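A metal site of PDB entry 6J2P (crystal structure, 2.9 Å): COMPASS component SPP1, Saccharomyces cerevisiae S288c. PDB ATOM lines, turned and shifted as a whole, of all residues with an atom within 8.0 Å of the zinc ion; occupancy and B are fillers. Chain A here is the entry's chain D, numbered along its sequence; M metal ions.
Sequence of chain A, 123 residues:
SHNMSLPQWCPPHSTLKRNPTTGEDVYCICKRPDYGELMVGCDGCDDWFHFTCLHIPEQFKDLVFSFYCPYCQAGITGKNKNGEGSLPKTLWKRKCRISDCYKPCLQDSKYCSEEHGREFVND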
ATOM      1  N   TYR A  27      10.865  -5.735 -11.257  1.00  0.00           N
ATOM      2  CA  TYR A  27      11.564  -6.974 -11.573  1.00  0.00           C
ATOM      3  C   TYR A  27      12.133  -7.614 -10.306  1.00  0.00           C
ATOM      4  O   TYR A  27      11.960  -7.114  -9.190  1.00  0.00           O
ATOM      5  CB  TYR A  27      12.688  -6.738 -12.585  1.00  0.00           C
ATOM      6  CG  TYR A  27      12.273  -6.074 -13.877  1.00  0.00           C
ATOM      7  CD1 TYR A  27      11.896  -6.824 -14.980  1.00  0.00           C
ATOM      8  CD2 TYR A  27      12.277  -4.689 -14.007  1.00  0.00           C
ATOM      9  CE1 TYR A  27      11.522  -6.221 -16.163  1.00  0.00           C
ATOM     10  CE2 TYR A  27      11.898  -4.070 -15.185  1.00  0.00           C
ATOM     11  CZ  TYR A  27      11.521  -4.850 -16.260  1.00  0.00           C
ATOM     12  OH  TYR A  27      11.152  -4.239 -17.442  1.00  0.00           O
ATOM     13  N   CYS A  28      12.828  -8.741 -10.502  1.00  0.00           N
ATOM     14  CA  CYS A  28      13.677  -9.391  -9.507  1.00  0.00           C
ATOM     15  C   CYS A  28      12.924  -9.850  -8.272  1.00  0.00           C
ATOM     16  O   CYS A  28      11.694  -9.722  -8.175  1.00  0.00           O
ATOM     17  CB  CYS A  28      14.829  -8.462  -9.104  1.00  0.00           C
ATOM     18  SG  CYS A  28      16.220  -9.292  -8.285  1.00  0.00           S
ATOM     19  N   ILE A  29      13.666 -10.412  -7.310  1.00  0.00           N
ATOM     20  CA  ILE A  29      13.060 -10.849  -6.046  1.00  0.00           C
ATOM     21  C   ILE A  29      12.924  -9.677  -5.082  1.00  0.00           C
ATOM     22  O   ILE A  29      12.056  -9.697  -4.199  1.00  0.00           O
ATOM     23  CB  ILE A  29      13.875 -11.991  -5.426  1.00  0.00           C
ATOM     24  CG1 ILE A  29      15.323 -11.551  -5.170  1.00  0.00           C
ATOM     25  CG2 ILE A  29      13.864 -13.209  -6.337  1.00  0.00           C
ATOM     26  CD1 ILE A  29      16.214 -12.657  -4.668  1.00  0.00           C
ATOM     27  N   CYS A  30      13.764  -8.650  -5.219  1.00  0.00           N
ATOM     28  CA  CYS A  30      13.620  -7.448  -4.409  1.00  0.00           C
ATOM     29  C   CYS A  30      12.392  -6.648  -4.780  1.00  0.00           C
ATOM     30  O   CYS A  30      12.002  -5.744  -4.021  1.00  0.00           O
ATOM     31  CB  CYS A  30      14.868  -6.575  -4.542  1.00  0.00           C
ATOM     32  SG  CYS A  30      15.042  -5.806  -6.180  1.00  0.00           S
ATOM     33  N   LYS A  31      11.774  -6.948  -5.926  1.00  0.00           N
ATOM     34  CA  LYS A  31      10.557  -6.270  -6.390  1.00  0.00           C
ATOM     35  C   LYS A  31      10.800  -4.772  -6.557  1.00  0.00           C
ATOM     36  O   LYS A  31       9.985  -3.930  -6.147  1.00  0.00           O
ATOM     37  CB  LYS A  31       9.381  -6.556  -5.460  1.00  0.00           C
ATOM     38  CG  LYS A  31       8.871  -7.974  -5.530  1.00  0.00           C
ATOM     39  CD  LYS A  31       8.068  -8.211  -6.806  1.00  0.00           C
ATOM     40  CE  LYS A  31       8.186  -9.647  -7.291  1.00  0.00           C
ATOM     41  NZ  LYS A  31       8.931  -9.751  -8.573  1.00  0.00           N
ATOM     42  N   ARG A  32      11.928  -4.433  -7.174  1.00  0.00           N
ATOM     43  CA  ARG A  32      12.298  -3.052  -7.473  1.00  0.00           C
ATOM     44  C   ARG A  32      12.417  -2.861  -8.986  1.00  0.00           C
ATOM     45  O   ARG A  32      12.684  -3.828  -9.709  1.00  0.00           O
ATOM     46  CB  ARG A  32      13.617  -2.665  -6.807  1.00  0.00           C
ATOM     47  CG  ARG A  32      13.587  -2.684  -5.288  1.00  0.00           C
ATOM     48  CD  ARG A  32      14.761  -1.915  -4.698  1.00  0.00           C
ATOM     49  NE  ARG A  32      15.992  -2.700  -4.686  1.00  0.00           N
ATOM     50  CZ  ARG A  32      16.958  -2.610  -5.605  1.00  0.00           C
ATOM     51  NH1 ARG A  32      16.812  -1.777  -6.619  1.00  0.00           N
ATOM     52  NH2 ARG A  32      18.041  -3.356  -5.512  1.00  0.00           N
ATOM     53  N   PRO A  33      12.211  -1.640  -9.480  1.00  0.00           N
ATOM     54  CA  PRO A  33      12.320  -1.412 -10.927  1.00  0.00           C
ATOM     55  C   PRO A  33      13.757  -1.471 -11.447  1.00  0.00           C
ATOM     56  O   PRO A  33      14.694  -1.696 -10.676  1.00  0.00           O
ATOM     57  CB  PRO A  33      11.729  -0.002 -11.109  1.00  0.00           C
ATOM     58  CG  PRO A  33      11.837   0.628  -9.769  1.00  0.00           C
ATOM     59  CD  PRO A  33      11.693  -0.476  -8.765  1.00  0.00           C
ATOM     60  N   GLU A  37      21.116  -0.843 -12.857  1.00  0.00           N
ATOM     61  CA  GLU A  37      22.091  -1.770 -12.285  1.00  0.00           C
ATOM     62  C   GLU A  37      22.162  -3.053 -13.113  1.00  0.00           C
ATOM     63  O   GLU A  37      21.288  -3.357 -13.928  1.00  0.00           O
ATOM     64  CB  GLU A  37      21.743  -2.080 -10.830  1.00  0.00           C
ATOM     65  CG  GLU A  37      20.365  -2.683 -10.631  1.00  0.00           C
ATOM     66  CD  GLU A  37      19.259  -1.644 -10.603  1.00  0.00           C
ATOM     67  OE1 GLU A  37      18.772  -1.306  -9.497  1.00  0.00           O
ATOM     68  OE2 GLU A  37      18.859  -1.164 -11.684  1.00  0.00           O
ATOM     69  N   LEU A  38      23.236  -3.813 -12.886  1.00  0.00           N
ATOM     70  CA  LEU A  38      23.490  -5.014 -13.680  1.00  0.00           C
ATOM     71  C   LEU A  38      22.506  -6.115 -13.326  1.00  0.00           C
ATOM     72  O   LEU A  38      22.290  -6.421 -12.146  1.00  0.00           O
ATOM     73  CB  LEU A  38      24.926  -5.491 -13.470  1.00  0.00           C
ATOM     74  CG  LEU A  38      25.299  -6.837 -14.092  1.00  0.00           C
ATOM     75  CD1 LEU A  38      25.101  -6.834 -15.599  1.00  0.00           C
ATOM     76  CD2 LEU A  38      26.735  -7.209 -13.735  1.00  0.00           C
ATOM     77  N   MET A  39      21.903  -6.713 -14.350  1.00  0.00           N
ATOM     78  CA  MET A  39      20.886  -7.734 -14.182  1.00  0.00           C
ATOM     79  C   MET A  39      21.167  -8.911 -15.103  1.00  0.00           C
ATOM     80  O   MET A  39      21.952  -8.829 -16.047  1.00  0.00           O
ATOM     81  CB  MET A  39      19.488  -7.185 -14.469  1.00  0.00           C
ATOM     82  CG  MET A  39      19.045  -6.093 -13.504  1.00  0.00           C
ATOM     83  SD  MET A  39      17.268  -6.127 -13.231  1.00  0.00           S
ATOM     84  CE  MET A  39      16.732  -5.021 -14.533  1.00  0.00           C
ATOM     85  N   TRP A  48      13.975 -10.659 -14.910  1.00  0.00           N
ATOM     86  CA  TRP A  48      15.349 -10.209 -14.757  1.00  0.00           C
ATOM     87  C   TRP A  48      15.656  -9.997 -13.288  1.00  0.00           C
ATOM     88  O   TRP A  48      14.800  -9.576 -12.510  1.00  0.00           O
ATOM     89  CB  TRP A  48      15.581  -8.925 -15.556  1.00  0.00           C
ATOM     90  CG  TRP A  48      15.405  -9.136 -17.022  1.00  0.00           C
ATOM     91  CD1 TRP A  48      14.228  -9.223 -17.706  1.00  0.00           C
ATOM     92  CD2 TRP A  48      16.449  -9.316 -17.997  1.00  0.00           C
ATOM     93  NE1 TRP A  48      14.468  -9.435 -19.039  1.00  0.00           N
ATOM     94  CE2 TRP A  48      15.821  -9.489 -19.252  1.00  0.00           C
ATOM     95  CE3 TRP A  48      17.841  -9.328 -17.933  1.00  0.00           C
ATOM     96  CZ2 TRP A  48      16.548  -9.684 -20.423  1.00  0.00           C
ATOM     97  CZ3 TRP A  48      18.558  -9.516 -19.100  1.00  0.00           C
ATOM     98  CH2 TRP A  48      17.911  -9.691 -20.329  1.00  0.00           C
ATOM     99  N   PHE A  49      16.897 -10.285 -12.902  1.00  0.00           N
ATOM    100  CA  PHE A  49      17.285 -10.332 -11.500  1.00  0.00           C
ATOM    101  C   PHE A  49      18.593  -9.597 -11.289  1.00  0.00           C
ATOM    102  O   PHE A  49      19.549  -9.765 -12.061  1.00  0.00           O
ATOM    103  CB  PHE A  49      17.398 -11.775 -11.004  1.00  0.00           C
ATOM    104  CG  PHE A  49      16.097 -12.522 -11.009  1.00  0.00           C
ATOM    105  CD1 PHE A  49      15.620 -13.108 -12.168  1.00  0.00           C
ATOM    106  CD2 PHE A  49      15.337 -12.630  -9.858  1.00  0.00           C
ATOM    107  CE1 PHE A  49      14.423 -13.794 -12.183  1.00  0.00           C
ATOM    108  CE2 PHE A  49      14.136 -13.314  -9.864  1.00  0.00           C
ATOM    109  CZ  PHE A  49      13.669 -13.894 -11.031  1.00  0.00           C
ATOM    110  N   HIS A  50      18.647  -8.779 -10.234  1.00  0.00           N
ATOM    111  CA  HIS A  50      19.861  -8.052  -9.907  1.00  0.00           C
ATOM    112  C   HIS A  50      20.968  -9.010  -9.470  1.00  0.00           C
ATOM    113  O   HIS A  50      20.718  -9.986  -8.752  1.00  0.00           O
ATOM    114  CB  HIS A  50      19.591  -7.041  -8.792  1.00  0.00           C
ATOM    115  CG  HIS A  50      18.545  -6.030  -9.134  1.00  0.00           C
ATOM    116  ND1 HIS A  50      17.518  -5.693  -8.272  1.00  0.00           N
ATOM    117  CD2 HIS A  50      18.367  -5.285 -10.245  1.00  0.00           C
ATOM    118  CE1 HIS A  50      16.755  -4.791  -8.843  1.00  0.00           C
ATOM    119  NE2 HIS A  50      17.246  -4.518 -10.037  1.00  0.00           N
ATOM    120  N   PHE A  51      22.187  -8.719  -9.902  1.00  0.00           N
ATOM    121  CA  PHE A  51      23.329  -9.515  -9.460  1.00  0.00           C
ATOM    122  C   PHE A  51      23.548  -9.366  -7.962  1.00  0.00           C
ATOM    123  O   PHE A  51      23.888 -10.327  -7.269  1.00  0.00           O
ATOM    124  CB  PHE A  51      24.580  -9.108 -10.224  1.00  0.00           C
ATOM    125  CG  PHE A  51      24.778  -9.857 -11.514  1.00  0.00           C
ATOM    126  CD1 PHE A  51      23.913  -9.684 -12.565  1.00  0.00           C
ATOM    127  CD2 PHE A  51      25.848 -10.735 -11.656  1.00  0.00           C
ATOM    128  CE1 PHE A  51      24.096 -10.374 -13.750  1.00  0.00           C
ATOM    129  CE2 PHE A  51      26.031 -11.425 -12.841  1.00  0.00           C
ATOM    130  CZ  PHE A  51      25.156 -11.244 -13.888  1.00  0.00           C
ATOM    131  N   THR A  52      23.340  -8.149  -7.429  1.00  0.00           N
ATOM    132  CA  THR A  52      23.538  -7.923  -6.001  1.00  0.00           C
ATOM    133  C   THR A  52      22.497  -8.668  -5.174  1.00  0.00           C
ATOM    134  O   THR A  52      22.775  -9.050  -4.023  1.00  0.00           O
ATOM    135  CB  THR A  52      23.489  -6.422  -5.698  1.00  0.00           C
ATOM    136  OG1 THR A  52      22.317  -5.849  -6.289  1.00  0.00           O
ATOM    137  CG2 THR A  52      24.719  -5.727  -6.240  1.00  0.00           C
ATOM    138  N   CYS A  53      21.305  -8.878  -5.728  1.00  0.00           N
ATOM    139  CA  CYS A  53      20.254  -9.567  -4.973  1.00  0.00           C
ATOM    140  C   CYS A  53      20.513 -11.073  -4.889  1.00  0.00           C
ATOM    141  O   CYS A  53      20.219 -11.693  -3.860  1.00  0.00           O
ATOM    142  CB  CYS A  53      18.895  -9.299  -5.620  1.00  0.00           C
ATOM    143  SG  CYS A  53      18.307  -7.590  -5.436  1.00  0.00           S
ATOM    144  N   LEU A  54      21.057 -11.667  -5.952  1.00  0.00           N
ATOM    145  CA  LEU A  54      21.401 -13.076  -5.938  1.00  0.00           C
ATOM    146  C   LEU A  54      22.775 -13.360  -5.336  1.00  0.00           C
ATOM    147  O   LEU A  54      23.229 -14.501  -5.382  1.00  0.00           O
ATOM    148  CB  LEU A  54      21.341 -13.642  -7.358  1.00  0.00           C
ATOM    149  CG  LEU A  54      20.079 -13.324  -8.162  1.00  0.00           C
ATOM    150  CD1 LEU A  54      20.415 -13.169  -9.625  1.00  0.00           C
ATOM    151  CD2 LEU A  54      19.030 -14.416  -7.950  1.00  0.00           C
HETATM  152 ZN    ZN M   1      16.714  -7.199  -7.107  1.00  0.00          ZN
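A ring nitrogen (NE2) of His 50 lies close to the side-chain sulfur (SD) of Met 39, 3.6 Å away.
SG of Cys 30 sits close to N of Arg 32 (3.5 Å).
The side-chain amino group (NZ) of Lys 31 lies within hydrogen-bond range of the backbone carbonyl oxygen (O) of Cys 28, at 2.8 Å.
The backbone NH of Cys 28 sits at hydrogen-bond distance from the backbone carbonyl oxygen of Trp 48 (2.9 Å).
The zinc ion is bound by ND1 of His 50 (2.1 Å), SG of Cys 53 (2.3 Å), SG of Cys 30 (2.4 Å) and SG of Cys 28 (2.5 Å).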
